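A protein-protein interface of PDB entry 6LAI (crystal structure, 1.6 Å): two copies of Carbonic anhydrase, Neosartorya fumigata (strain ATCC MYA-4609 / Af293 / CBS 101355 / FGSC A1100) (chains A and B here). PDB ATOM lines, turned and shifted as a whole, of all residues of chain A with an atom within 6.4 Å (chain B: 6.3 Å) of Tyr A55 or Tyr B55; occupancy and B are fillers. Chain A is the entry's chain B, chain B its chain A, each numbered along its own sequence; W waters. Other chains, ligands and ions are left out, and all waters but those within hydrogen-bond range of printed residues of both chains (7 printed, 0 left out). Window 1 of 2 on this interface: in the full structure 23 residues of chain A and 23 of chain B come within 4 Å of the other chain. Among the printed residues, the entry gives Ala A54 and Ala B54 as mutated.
Water W1 lies within hydrogen-bond range of OG of Ser B67 (2.4 Å) and OH of Tyr A55 (2.5 Å).
Water W2 lies within hydrogen-bond range of N of Leu A58 and OG1 of Thr B71.
Water W4 lies within hydrogen-bond range of the backbone NH of Leu B58 (2.9 Å) and the side-chain hydroxyl of Thr A71 (3.0 Å).
Of the 19 printed residues of chain B, 9 touch a printed residue of chain A.
Printed residues of chain B that touch a printed residue of chain A: Ser B35, Phe B53, Ala B54, Tyr B55, Arg B56, Leu B58, Asp B65, Ser B67 and Thr B71.
Of the 19 printed residues of chain A, 9 touch a printed residue of chain B.
Ser A35 touches Phe B53, and with the chains exchanged Phe A53 touches Ser B35.
Leu A58 touches Thr B71, and with the chains exchanged Thr A71 touches Leu B58.
Asp A65 touches its own counterpart, Asp B65.
Asp A65 touches Ser B67, and with the chains exchanged Ser A67 touches Asp B65.
Of the printed residues of chain B, Ala A54 touches Ser B35 and Arg B56.
Of chain B, only Tyr B55, Arg B56 and Ser B67 come within 4 Å of Tyr A55.
Of the printed residues of chain B, Asp A65 touches Asp B65 (3.2 Å) and Ser B67 (2.5 Å).
Of the printed residues of chain B, Ser A67 touches Tyr B55 (3.9 Å), Asp B65 (2.7 Å) and Ser B67 (3.7 Å).
Printed residues of chain A within 4 Å of Phe B53: Ser A35 and Leu A58.
Tyr B55 touches just these residues of chain A: Tyr A55, Arg A56 and Ser A67.
The nearest residue of chain A that does not touch Tyr B55 is Ser A35 (4.2 Å).
Among the printed residues, merely in contact across the chains: Ser A35 with Phe B53 (3.5 Å), Phe A53 with Ser B35 (3.5 Å), Phe A53 with Leu B58 (3.9 Å), Ala A54 with Arg B56 (3.5 Å), Tyr A55 with Arg B56 (3.2 Å), Tyr A55 with Ser B67 (3.7 Å), Arg A56 with Ala B54 (3.6 Å), Arg A56 with Tyr B55 (3.2 Å), Leu A58 with Phe B53 (3.8 Å), Leu A58 with Thr B71 (3.7 Å), Ser A67 with Tyr B55 (3.9 Å), Ser A67 with Ser B67 (3.7 Å) and Thr A71 with Leu B58 (3.9 Å).
The side-chain hydroxyl of Ser B35 sits at hydrogen-bond distance from the backbone carbonyl oxygen of Ala A54 (2.8 Å).
The side-chain hydroxyl (OG) of Ser A35 is in hydrogen-bond range of the backbone carbonyl oxygen (O) of Ala B54 (2.7 Å).
OH of Tyr B55 sits at hydrogen-bond distance from OH of Tyr A55 (2.9 Å).
The backbone NH of Arg B56 sits at hydrogen-bond distance from the backbone carbonyl oxygen of Arg A56 (3.1 Å).
The side-chain carboxylate (OD2) of Asp B65 lies within hydrogen-bond range of the backbone NH (N) of Ser A67, at 2.7 Å.
The side-chain hydroxyl (OG) of Ser B67 sits at hydrogen-bond distance from the side-chain carboxylate (OD2) of Asp A65 (2.5 Å).
The side-chain carboxylate of Asp A65 lies close to the side-chain carboxylate of Asp B65, at 3.2 Å.
The backbone NH (N) of Trp B31 lies within hydrogen-bond range of the backbone carbonyl oxygen (O) of Phe B53 (2.9 Å).
The backbone carbonyl oxygen (O) of Cys A34 lies within hydrogen-bond range of the guanidinium group (NH1) of Arg A56 (2.9 Å).
The backbone carbonyl oxygen (O) of Ser A67 lies within hydrogen-bond range of the side-chain hydroxyl (OG1) of Thr A71.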
ATOM      1  N   LEU A  30       1.508 -38.145  18.137  1.00  0.00           N
ATOM      2  CA  LEU A  30       1.470 -36.746  17.673  1.00  0.00           C
ATOM      3  C   LEU A  30       2.876 -36.199  17.813  1.00  0.00           C
ATOM      4  O   LEU A  30       3.417 -36.125  18.921  1.00  0.00           O
ATOM      5  CB  LEU A  30       0.467 -35.916  18.478  1.00  0.00           C
ATOM      6  CG  LEU A  30       0.493 -34.409  18.292  1.00  0.00           C
ATOM      7  CD1 LEU A  30       0.245 -34.018  16.819  1.00  0.00           C
ATOM      8  CD2 LEU A  30      -0.528 -33.719  19.158  1.00  0.00           C
ATOM      9  N   TRP A  31       3.463 -35.807  16.688  1.00  0.00           N
ATOM     10  CA  TRP A  31       4.833 -35.305  16.591  1.00  0.00           C
ATOM     11  C   TRP A  31       4.760 -33.830  16.274  1.00  0.00           C
ATOM     12  O   TRP A  31       4.180 -33.481  15.238  1.00  0.00           O
ATOM     13  CB  TRP A  31       5.581 -36.030  15.457  1.00  0.00           C
ATOM     14  CG  TRP A  31       7.022 -35.644  15.389  1.00  0.00           C
ATOM     15  CD1 TRP A  31       7.575 -34.600  14.704  1.00  0.00           C
ATOM     16  CD2 TRP A  31       8.113 -36.323  16.014  1.00  0.00           C
ATOM     17  NE1 TRP A  31       8.932 -34.602  14.863  1.00  0.00           N
ATOM     18  CE2 TRP A  31       9.283 -35.617  15.713  1.00  0.00           C
ATOM     19  CE3 TRP A  31       8.163 -37.465  16.841  1.00  0.00           C
ATOM     20  CZ2 TRP A  31      10.548 -36.091  16.117  1.00  0.00           C
ATOM     21  CZ3 TRP A  31       9.397 -37.873  17.301  1.00  0.00           C
ATOM     22  CH2 TRP A  31      10.554 -37.191  16.945  1.00  0.00           C
ATOM     23  N   ILE A  32       5.226 -32.973  17.191  1.00  0.00           N
ATOM     24  CA  ILE A  32       5.213 -31.509  16.996  1.00  0.00           C
ATOM     25  C   ILE A  32       6.635 -31.083  16.684  1.00  0.00           C
ATOM     26  O   ILE A  32       7.538 -31.212  17.538  1.00  0.00           O
ATOM     27  CB  ILE A  32       4.641 -30.793  18.223  1.00  0.00           C
ATOM     28  CG1 ILE A  32       3.191 -31.281  18.456  1.00  0.00           C
ATOM     29  CG2 ILE A  32       4.787 -29.288  18.020  1.00  0.00           C
ATOM     30  CD1 ILE A  32       2.658 -30.968  19.839  1.00  0.00           C
ATOM     31  N   GLY A  33       6.885 -30.677  15.435  1.00  0.00           N
ATOM     32  CA  GLY A  33       8.215 -30.297  14.973  1.00  0.00           C
ATOM     33  C   GLY A  33       8.179 -28.913  14.360  1.00  0.00           C
ATOM     34  O   GLY A  33       7.101 -28.307  14.294  1.00  0.00           O
ATOM     35  N   CYS A  34       9.335 -28.398  13.962  1.00  0.00           N
ATOM     36  CA  CYS A  34       9.455 -27.013  13.456  1.00  0.00           C
ATOM     37  C   CYS A  34       9.450 -26.955  11.920  1.00  0.00           C
ATOM     38  O   CYS A  34      10.116 -27.766  11.245  1.00  0.00           O
ATOM     39  CB  CYS A  34      10.718 -26.395  14.015  1.00  0.00           C
ATOM     40  SG  CYS A  34      10.946 -24.647  13.539  1.00  0.00           S
ATOM     41  N   SER A  35       8.812 -25.891  11.418  1.00  0.00           N
ATOM     42  CA  SER A  35       8.757 -25.599   9.976  1.00  0.00           C
ATOM     43  C   SER A  35      10.135 -25.438   9.335  1.00  0.00           C
ATOM     44  O   SER A  35      10.237 -25.710   8.134  1.00  0.00           O
ATOM     45  CB  SER A  35       7.913 -24.408   9.775  1.00  0.00           C
ATOM     46  OG  SER A  35       6.570 -24.628  10.238  1.00  0.00           O
ATOM     47  N   PHE A  53       1.814 -38.867  13.252  1.00  0.00           N
ATOM     48  CA  PHE A  53       0.809 -37.829  12.942  1.00  0.00           C
ATOM     49  C   PHE A  53       1.497 -36.519  13.299  1.00  0.00           C
ATOM     50  O   PHE A  53       1.663 -36.234  14.477  1.00  0.00           O
ATOM     51  CB  PHE A  53      -0.475 -38.050  13.741  1.00  0.00           C
ATOM     52  CG  PHE A  53      -1.587 -37.106  13.438  1.00  0.00           C
ATOM     53  CD1 PHE A  53      -2.339 -37.216  12.266  1.00  0.00           C
ATOM     54  CD2 PHE A  53      -1.838 -36.032  14.290  1.00  0.00           C
ATOM     55  CE1 PHE A  53      -3.388 -36.347  12.035  1.00  0.00           C
ATOM     56  CE2 PHE A  53      -2.898 -35.174  14.061  1.00  0.00           C
ATOM     57  CZ  PHE A  53      -3.658 -35.319  12.919  1.00  0.00           C
ATOM     58  N   ALA A  54       1.874 -35.727  12.303  1.00  0.00           N
ATOM     59  CA  ALA A  54       2.849 -34.644  12.496  1.00  0.00           C
ATOM     60  C   ALA A  54       2.176 -33.298  12.356  1.00  0.00           C
ATOM     61  O   ALA A  54       1.463 -33.042  11.355  1.00  0.00           O
ATOM     62  CB  ALA A  54       3.974 -34.767  11.490  1.00  0.00           C
ATOM     63  N   TYR A  55       2.377 -32.430  13.339  1.00  0.00           N
ATOM     64  CA  TYR A  55       2.039 -31.016  13.284  1.00  0.00           C
ATOM     65  C   TYR A  55       3.349 -30.259  13.237  1.00  0.00           C
ATOM     66  O   TYR A  55       4.184 -30.366  14.136  1.00  0.00           O
ATOM     67  CB  TYR A  55       1.181 -30.616  14.505  1.00  0.00           C
ATOM     68  CG  TYR A  55       0.720 -29.201  14.448  1.00  0.00           C
ATOM     69  CD1 TYR A  55      -0.117 -28.780  13.428  1.00  0.00           C
ATOM     70  CD2 TYR A  55       1.200 -28.234  15.307  1.00  0.00           C
ATOM     71  CE1 TYR A  55      -0.492 -27.442  13.309  1.00  0.00           C
ATOM     72  CE2 TYR A  55       0.786 -26.904  15.246  1.00  0.00           C
ATOM     73  CZ  TYR A  55      -0.041 -26.492  14.203  1.00  0.00           C
ATOM     74  OH  TYR A  55      -0.446 -25.179  14.085  1.00  0.00           O
ATOM     75  N   ARG A  56       3.577 -29.538  12.151  1.00  0.00           N
ATOM     76  CA  ARG A  56       4.870 -28.875  11.945  1.00  0.00           C
ATOM     77  C   ARG A  56       4.576 -27.385  11.844  1.00  0.00           C
ATOM     78  O   ARG A  56       3.878 -26.970  10.940  1.00  0.00           O
ATOM     79  CB  ARG A  56       5.603 -29.396  10.719  1.00  0.00           C
ATOM     80  CG  ARG A  56       7.043 -28.916  10.631  1.00  0.00           C
ATOM     81  CD  ARG A  56       7.868 -29.629   9.586  1.00  0.00           C
ATOM     82  NE  ARG A  56       8.066 -31.019   9.892  1.00  0.00           N
ATOM     83  CZ  ARG A  56       8.883 -31.495  10.824  1.00  0.00           C
ATOM     84  NH1 ARG A  56       9.665 -30.647  11.534  1.00  0.00           N
ATOM     85  NH2 ARG A  56       8.876 -32.805  11.076  1.00  0.00           N
ATOM     86  N   SER A  57       5.153 -26.635  12.777  1.00  0.00           N
ATOM     87  CA  SER A  57       4.720 -25.268  13.116  1.00  0.00           C
ATOM     88  C   SER A  57       5.914 -24.367  13.386  1.00  0.00           C
ATOM     89  O   SER A  57       7.017 -24.862  13.527  1.00  0.00           O
ATOM     90  CB  SER A  57       3.885 -25.315  14.369  1.00  0.00           C
ATOM     91  OG  SER A  57       4.678 -25.768  15.487  1.00  0.00           O
ATOM     92  N   LEU A  58       5.645 -23.067  13.463  1.00  0.00           N
ATOM     93  CA  LEU A  58       6.722 -22.121  13.820  1.00  0.00           C
ATOM     94  C   LEU A  58       7.337 -22.498  15.162  1.00  0.00           C
ATOM     95  O   LEU A  58       6.624 -22.488  16.174  1.00  0.00           O
ATOM     96  CB  LEU A  58       6.180 -20.702  13.883  1.00  0.00           C
ATOM     97  CG  LEU A  58       5.560 -20.147  12.618  1.00  0.00           C
ATOM     98  CD1 LEU A  58       4.862 -18.837  12.935  1.00  0.00           C
ATOM     99  CD2 LEU A  58       6.610 -19.972  11.543  1.00  0.00           C
ATOM    100  N   ASN A  60       8.279 -25.212  16.527  1.00  0.00           N
ATOM    101  CA  ASN A  60       7.749 -26.435  17.202  1.00  0.00           C
ATOM    102  C   ASN A  60       6.992 -25.961  18.450  1.00  0.00           C
ATOM    103  O   ASN A  60       7.114 -26.598  19.515  1.00  0.00           O
ATOM    104  CB  ASN A  60       8.840 -27.502  17.420  1.00  0.00           C
ATOM    105  CG  ASN A  60      10.102 -27.049  18.135  1.00  0.00           C
ATOM    106  OD1 ASN A  60      11.062 -26.628  17.460  1.00  0.00           O
ATOM    107  ND2 ASN A  60      10.083 -27.108  19.484  1.00  0.00           N
ATOM    108  N   MET A  61       6.185 -24.907  18.345  1.00  0.00           N
ATOM    109  CA  MET A  61       5.387 -24.389  19.450  1.00  0.00           C
ATOM    110  C   MET A  61       3.925 -24.789  19.286  1.00  0.00           C
ATOM    111  O   MET A  61       3.434 -25.018  18.166  1.00  0.00           O
ATOM    112  CB  MET A  61       5.508 -22.873  19.562  1.00  0.00           C
ATOM    113  CG  MET A  61       6.863 -22.411  19.783  1.00  0.00           C
ATOM    114  SD  MET A  61       6.707 -20.620  20.158  1.00  0.00           S
ATOM    115  CE  MET A  61       8.425 -20.193  20.113  1.00  0.00           C
ATOM    116  N   MET A  62       3.234 -24.893  20.408  1.00  0.00           N
ATOM    117  CA  MET A  62       1.751 -24.925  20.461  1.00  0.00           C
ATOM    118  C   MET A  62       1.351 -23.688  21.245  1.00  0.00           C
ATOM    119  O   MET A  62       1.743 -23.543  22.445  1.00  0.00           O
ATOM    120  CB  MET A  62       1.214 -26.164  21.160  1.00  0.00           C
ATOM    121  CG  MET A  62       1.665 -27.431  20.508  1.00  0.00           C
ATOM    122  SD  MET A  62       0.734 -27.690  18.963  1.00  0.00           S
ATOM    123  CE  MET A  62      -0.606 -28.633  19.695  1.00  0.00           C
ATOM    124  N   ASP A  65      -4.310 -21.155  20.339  1.00  0.00           N
ATOM    125  CA  ASP A  65      -5.121 -20.695  19.196  1.00  0.00           C
ATOM    126  C   ASP A  65      -5.976 -21.856  18.695  1.00  0.00           C
ATOM    127  O   ASP A  65      -5.930 -22.956  19.299  1.00  0.00           O
ATOM    128  CB  ASP A  65      -4.202 -20.074  18.154  1.00  0.00           C
ATOM    129  CG  ASP A  65      -3.395 -21.084  17.361  1.00  0.00           C
ATOM    130  OD1 ASP A  65      -3.263 -22.258  17.808  1.00  0.00           O
ATOM    131  OD2 ASP A  65      -2.906 -20.654  16.315  1.00  0.00           O
ATOM    132  N   SER A  67      -5.810 -23.581  15.905  1.00  0.00           N
ATOM    133  CA  SER A  67      -5.001 -24.674  15.317  1.00  0.00           C
ATOM    134  C   SER A  67      -4.447 -25.578  16.429  1.00  0.00           C
ATOM    135  O   SER A  67      -4.581 -26.812  16.287  1.00  0.00           O
ATOM    136  CB  SER A  67      -3.936 -24.138  14.417  1.00  0.00           C
ATOM    137  OG  SER A  67      -4.519 -23.574  13.272  1.00  0.00           O
ATOM    138  N   CYS A  68      -3.862 -25.051  17.518  1.00  0.00           N
ATOM    139  CA  CYS A  68      -3.337 -25.904  18.644  1.00  0.00           C
ATOM    140  C   CYS A  68      -4.476 -26.736  19.193  1.00  0.00           C
ATOM    141  O   CYS A  68      -4.342 -27.971  19.251  1.00  0.00           O
ATOM    142  CB  CYS A  68      -2.801 -25.217  19.919  1.00  0.00           C
ATOM    143  SG  CYS A  68      -2.608 -26.253  21.439  1.00  0.00           S
ATOM    144  N   THR A  71      -5.880 -29.439  16.681  1.00  0.00           N
ATOM    145  CA  THR A  71      -4.910 -30.490  16.352  1.00  0.00           C
ATOM    146  C   THR A  71      -4.832 -31.444  17.547  1.00  0.00           C
ATOM    147  O   THR A  71      -4.863 -32.642  17.362  1.00  0.00           O
ATOM    148  CB  THR A  71      -3.553 -29.894  15.953  1.00  0.00           C
ATOM    149  OG1 THR A  71      -3.791 -29.066  14.823  1.00  0.00           O
ATOM    150  CG2 THR A  71      -2.506 -30.938  15.625  1.00  0.00           C
ATOM    151  N   LEU B  30       7.199 -22.392   0.765  1.00  0.00           N
ATOM    152  CA  LEU B  30       6.295 -22.758   1.872  1.00  0.00           C
ATOM    153  C   LEU B  30       5.469 -23.935   1.377  1.00  0.00           C
ATOM    154  O   LEU B  30       4.705 -23.820   0.393  1.00  0.00           O
ATOM    155  CB  LEU B  30       5.389 -21.580   2.229  1.00  0.00           C
ATOM    156  CG  LEU B  30       4.253 -21.878   3.205  1.00  0.00           C
ATOM    157  CD1 LEU B  30       4.727 -22.438   4.539  1.00  0.00           C
ATOM    158  CD2 LEU B  30       3.410 -20.633   3.423  1.00  0.00           C
ATOM    159  N   TRP B  31       5.605 -25.066   2.080  1.00  0.00           N
ATOM    160  CA  TRP B  31       4.942 -26.326   1.708  1.00  0.00           C
ATOM    161  C   TRP B  31       3.863 -26.569   2.759  1.00  0.00           C
ATOM    162  O   TRP B  31       4.221 -26.688   3.963  1.00  0.00           O
ATOM    163  CB  TRP B  31       5.966 -27.446   1.682  1.00  0.00           C
ATOM    164  CG  TRP B  31       5.391 -28.742   1.242  1.00  0.00           C
ATOM    165  CD1 TRP B  31       4.760 -29.698   1.976  1.00  0.00           C
ATOM    166  CD2 TRP B  31       5.481 -29.238  -0.096  1.00  0.00           C
ATOM    167  NE1 TRP B  31       4.416 -30.746   1.161  1.00  0.00           N
ATOM    168  CE2 TRP B  31       4.772 -30.460  -0.126  1.00  0.00           C
ATOM    169  CE3 TRP B  31       6.025 -28.707  -1.268  1.00  0.00           C
ATOM    170  CZ2 TRP B  31       4.760 -31.258  -1.279  1.00  0.00           C
ATOM    171  CZ3 TRP B  31       5.937 -29.465  -2.416  1.00  0.00           C
ATOM    172  CH2 TRP B  31       5.305 -30.703  -2.412  1.00  0.00           C
ATOM    173  N   ILE B  32       2.620 -26.579   2.324  1.00  0.00           N
ATOM    174  CA  ILE B  32       1.478 -26.844   3.238  1.00  0.00           C
ATOM    175  C   ILE B  32       1.026 -28.257   2.970  1.00  0.00           C
ATOM    176  O   ILE B  32       0.496 -28.547   1.891  1.00  0.00           O
ATOM    177  CB  ILE B  32       0.375 -25.797   3.058  1.00  0.00           C
ATOM    178  CG1 ILE B  32       0.967 -24.399   3.283  1.00  0.00           C
ATOM    179  CG2 ILE B  32      -0.795 -26.161   3.948  1.00  0.00           C
ATOM    180  CD1 ILE B  32       0.067 -23.280   2.884  1.00  0.00           C
ATOM    181  N   GLY B  33       1.221 -29.146   3.946  1.00  0.00           N
ATOM    182  CA  GLY B  33       0.876 -30.563   3.809  1.00  0.00           C
ATOM    183  C   GLY B  33       0.002 -30.980   4.962  1.00  0.00           C
ATOM    184  O   GLY B  33      -0.273 -30.190   5.873  1.00  0.00           O
ATOM    185  N   CYS B  34      -0.446 -32.212   4.921  1.00  0.00           N
ATOM    186  CA  CYS B  34      -1.358 -32.780   5.946  1.00  0.00           C
ATOM    187  C   CYS B  34      -0.635 -33.613   7.002  1.00  0.00           C
ATOM    188  O   CYS B  34       0.243 -34.417   6.695  1.00  0.00           O
ATOM    189  CB  CYS B  34      -2.445 -33.594   5.266  1.00  0.00           C
ATOM    190  SG  CYS B  34      -3.714 -34.255   6.381  1.00  0.00           S
ATOM    191  N   SER B  35      -1.110 -33.436   8.232  1.00  0.00           N
ATOM    192  CA  SER B  35      -0.655 -34.179   9.415  1.00  0.00           C
ATOM    193  C   SER B  35      -0.798 -35.686   9.290  1.00  0.00           C
ATOM    194  O   SER B  35       0.091 -36.351   9.844  1.00  0.00           O
ATOM    195  CB  SER B  35      -1.381 -33.690  10.659  1.00  0.00           C
ATOM    196  OG  SER B  35      -1.140 -32.314  10.825  1.00  0.00           O
ATOM    197  N   PHE B  53      10.248 -25.130   3.600  1.00  0.00           N
ATOM    198  CA  PHE B  53       9.714 -24.560   4.859  1.00  0.00           C
ATOM    199  C   PHE B  53       8.301 -25.094   4.984  1.00  0.00           C
ATOM    200  O   PHE B  53       7.410 -24.649   4.274  1.00  0.00           O
ATOM    201  CB  PHE B  53       9.812 -23.037   4.838  1.00  0.00           C
ATOM    202  CG  PHE B  53       9.373 -22.359   6.094  1.00  0.00           C
ATOM    203  CD1 PHE B  53      10.236 -22.281   7.183  1.00  0.00           C
ATOM    204  CD2 PHE B  53       8.102 -21.822   6.197  1.00  0.00           C
ATOM    205  CE1 PHE B  53       9.780 -21.701   8.349  1.00  0.00           C
ATOM    206  CE2 PHE B  53       7.687 -21.187   7.365  1.00  0.00           C
ATOM    207  CZ  PHE B  53       8.547 -21.125   8.423  1.00  0.00           C
ATOM    208  N   ALA B  54       8.102 -26.069   5.878  1.00  0.00           N
ATOM    209  CA  ALA B  54       6.887 -26.887   5.866  1.00  0.00           C
ATOM    210  C   ALA B  54       5.959 -26.492   7.009  1.00  0.00           C
ATOM    211  O   ALA B  54       6.387 -26.436   8.175  1.00  0.00           O
ATOM    212  CB  ALA B  54       7.229 -28.338   5.938  1.00  0.00           C
ATOM    213  N   TYR B  55       4.687 -26.275   6.691  1.00  0.00           N
ATOM    214  CA  TYR B  55       3.581 -26.154   7.653  1.00  0.00           C
ATOM    215  C   TYR B  55       2.718 -27.393   7.438  1.00  0.00           C
ATOM    216  O   TYR B  55       2.181 -27.588   6.336  1.00  0.00           O
ATOM    217  CB  TYR B  55       2.824 -24.845   7.445  1.00  0.00           C
ATOM    218  CG  TYR B  55       1.739 -24.639   8.463  1.00  0.00           C
ATOM    219  CD1 TYR B  55       2.081 -24.518   9.801  1.00  0.00           C
ATOM    220  CD2 TYR B  55       0.407 -24.674   8.147  1.00  0.00           C
ATOM    221  CE1 TYR B  55       1.108 -24.386  10.777  1.00  0.00           C
ATOM    222  CE2 TYR B  55      -0.583 -24.550   9.109  1.00  0.00           C
ATOM    223  CZ  TYR B  55      -0.225 -24.422  10.445  1.00  0.00           C
ATOM    224  OH  TYR B  55      -1.159 -24.267  11.440  1.00  0.00           O
ATOM    225  N   ARG B  56       2.608 -28.227   8.455  1.00  0.00           N
ATOM    226  CA  ARG B  56       1.884 -29.505   8.317  1.00  0.00           C
ATOM    227  C   ARG B  56       0.736 -29.498   9.300  1.00  0.00           C
ATOM    228  O   ARG B  56       0.976 -29.390  10.527  1.00  0.00           O
ATOM    229  CB  ARG B  56       2.808 -30.709   8.476  1.00  0.00           C
ATOM    230  CG  ARG B  56       2.161 -32.001   8.053  1.00  0.00           C
ATOM    231  CD  ARG B  56       3.080 -33.179   7.976  1.00  0.00           C
ATOM    232  NE  ARG B  56       4.050 -33.039   6.932  1.00  0.00           N
ATOM    233  CZ  ARG B  56       3.790 -33.126   5.621  1.00  0.00           C
ATOM    234  NH1 ARG B  56       2.596 -33.523   5.212  1.00  0.00           N
ATOM    235  NH2 ARG B  56       4.742 -32.934   4.735  1.00  0.00           N
ATOM    236  N   SER B  57      -0.459 -29.543   8.748  1.00  0.00           N
ATOM    237  CA  SER B  57      -1.699 -29.152   9.466  1.00  0.00           C
ATOM    238  C   SER B  57      -2.841 -30.109   9.165  1.00  0.00           C
ATOM    239  O   SER B  57      -2.743 -30.960   8.240  1.00  0.00           O
ATOM    240  CB  SER B  57      -2.117 -27.767   8.996  1.00  0.00           C
ATOM    241  OG  SER B  57      -2.454 -27.810   7.599  1.00  0.00           O
ATOM    242  N   LEU B  58      -3.921 -30.002   9.905  1.00  0.00           N
ATOM    243  CA  LEU B  58      -5.126 -30.824   9.608  1.00  0.00           C
ATOM    244  C   LEU B  58      -5.602 -30.583   8.174  1.00  0.00           C
ATOM    245  O   LEU B  58      -5.980 -29.456   7.841  1.00  0.00           O
ATOM    246  CB  LEU B  58      -6.236 -30.434  10.585  1.00  0.00           C
ATOM    247  CG  LEU B  58      -5.940 -30.685  12.048  1.00  0.00           C
ATOM    248  CD1 LEU B  58      -7.071 -30.117  12.892  1.00  0.00           C
ATOM    249  CD2 LEU B  58      -5.769 -32.136  12.345  1.00  0.00           C
ATOM    250  N   ASN B  60      -4.174 -30.334   5.364  1.00  0.00           N
ATOM    251  CA  ASN B  60      -3.383 -29.403   4.509  1.00  0.00           C
ATOM    252  C   ASN B  60      -4.242 -28.163   4.261  1.00  0.00           C
ATOM    253  O   ASN B  60      -4.280 -27.605   3.138  1.00  0.00           O
ATOM    254  CB  ASN B  60      -2.839 -30.080   3.236  1.00  0.00           C
ATOM    255  CG  ASN B  60      -3.841 -30.824   2.377  1.00  0.00           C
ATOM    256  OD1 ASN B  60      -4.011 -32.015   2.612  1.00  0.00           O
ATOM    257  ND2 ASN B  60      -4.506 -30.150   1.424  1.00  0.00           N
ATOM    258  N   MET B  61      -4.894 -27.650   5.303  1.00  0.00           N
ATOM    259  CA  MET B  61      -5.716 -26.429   5.206  1.00  0.00           C
ATOM    260  C   MET B  61      -5.018 -25.252   5.858  1.00  0.00           C
ATOM    261  O   MET B  61      -4.113 -25.416   6.699  1.00  0.00           O
ATOM    262  CB  MET B  61      -7.062 -26.603   5.900  1.00  0.00           C
ATOM    263  CG  MET B  61      -7.866 -27.712   5.345  1.00  0.00           C
ATOM    264  SD  MET B  61      -9.565 -27.576   6.048  1.00  0.00           S
ATOM    265  CE  MET B  61     -10.249 -29.121   5.511  1.00  0.00           C
ATOM    266  N   MET B  62      -5.395 -24.075   5.369  1.00  0.00           N
ATOM    267  CA  MET B  62      -5.092 -22.774   5.979  1.00  0.00           C
ATOM    268  C   MET B  62      -6.449 -22.149   6.275  1.00  0.00           C
ATOM    269  O   MET B  62      -7.285 -22.032   5.350  1.00  0.00           O
ATOM    270  CB  MET B  62      -4.286 -21.878   5.035  1.00  0.00           C
ATOM    271  CG  MET B  62      -2.969 -22.480   4.706  1.00  0.00           C
ATOM    272  SD  MET B  62      -1.825 -22.416   6.119  1.00  0.00           S
ATOM    273  CE  MET B  62      -1.199 -20.777   5.737  1.00  0.00           C
ATOM    274  N   ASP B  65      -7.035 -18.375  11.300  1.00  0.00           N
ATOM    275  CA  ASP B  65      -6.582 -18.564  12.694  1.00  0.00           C
ATOM    276  C   ASP B  65      -5.225 -17.889  12.843  1.00  0.00           C
ATOM    277  O   ASP B  65      -4.617 -17.525  11.803  1.00  0.00           O
ATOM    278  CB  ASP B  65      -6.674 -20.057  12.989  1.00  0.00           C
ATOM    279  CG  ASP B  65      -6.261 -20.435  14.378  1.00  0.00           C
ATOM    280  OD1 ASP B  65      -6.787 -19.790  15.329  1.00  0.00           O
ATOM    281  OD2 ASP B  65      -5.457 -21.366  14.484  1.00  0.00           O
ATOM    282  N   SER B  67      -2.358 -19.146  13.768  1.00  0.00           N
ATOM    283  CA  SER B  67      -1.251 -20.006  13.292  1.00  0.00           C
ATOM    284  C   SER B  67      -1.130 -19.821  11.764  1.00  0.00           C
ATOM    285  O   SER B  67      -0.011 -19.583  11.266  1.00  0.00           O
ATOM    286  CB  SER B  67      -1.458 -21.435  13.698  1.00  0.00           C
ATOM    287  OG  SER B  67      -1.008 -21.635  15.026  1.00  0.00           O
ATOM    288  N   CYS B  68      -2.224 -19.855  11.049  1.00  0.00           N
ATOM    289  CA  CYS B  68      -2.173 -19.832   9.569  1.00  0.00           C
ATOM    290  C   CYS B  68      -1.695 -18.427   9.149  1.00  0.00           C
ATOM    291  O   CYS B  68      -0.724 -18.303   8.375  1.00  0.00           O
ATOM    292  CB  CYS B  68      -3.515 -20.298   9.034  1.00  0.00           C
ATOM    293  SG  CYS B  68      -3.946 -22.001   9.521  1.00  0.00           S
ATOM    294  N   THR B  71       2.133 -17.916  10.153  1.00  0.00           N
ATOM    295  CA  THR B  71       3.005 -18.781   9.319  1.00  0.00           C
ATOM    296  C   THR B  71       3.142 -18.161   7.925  1.00  0.00           C
ATOM    297  O   THR B  71       4.286 -18.047   7.437  1.00  0.00           O
ATOM    298  CB  THR B  71       2.467 -20.206   9.268  1.00  0.00           C
ATOM    299  OG1 THR B  71       2.436 -20.660  10.620  1.00  0.00           O
ATOM    300  CG2 THR B  71       3.340 -21.133   8.448  1.00  0.00           C
HETATM  301  O   HOH W   1       0.843 -23.168  14.806  1.00  0.00           O
HETATM  302  O   HOH W   2       3.006 -22.377  12.874  1.00  0.00           O
HETATM  303  O   HOH W   3       6.620 -33.873   9.145  1.00  0.00           O
HETATM  304  O   HOH W   4      -3.615 -28.030  12.064  1.00  0.00           O
HETATM  305  O   HOH W   5      10.718 -28.305   6.419  1.00  0.00           O
HETATM  306  O   HOH W   6      -3.610 -25.147  11.304  1.00  0.00           O
HETATM  307  O   HOH W   7       7.084 -31.914   6.802  1.00  0.00           O
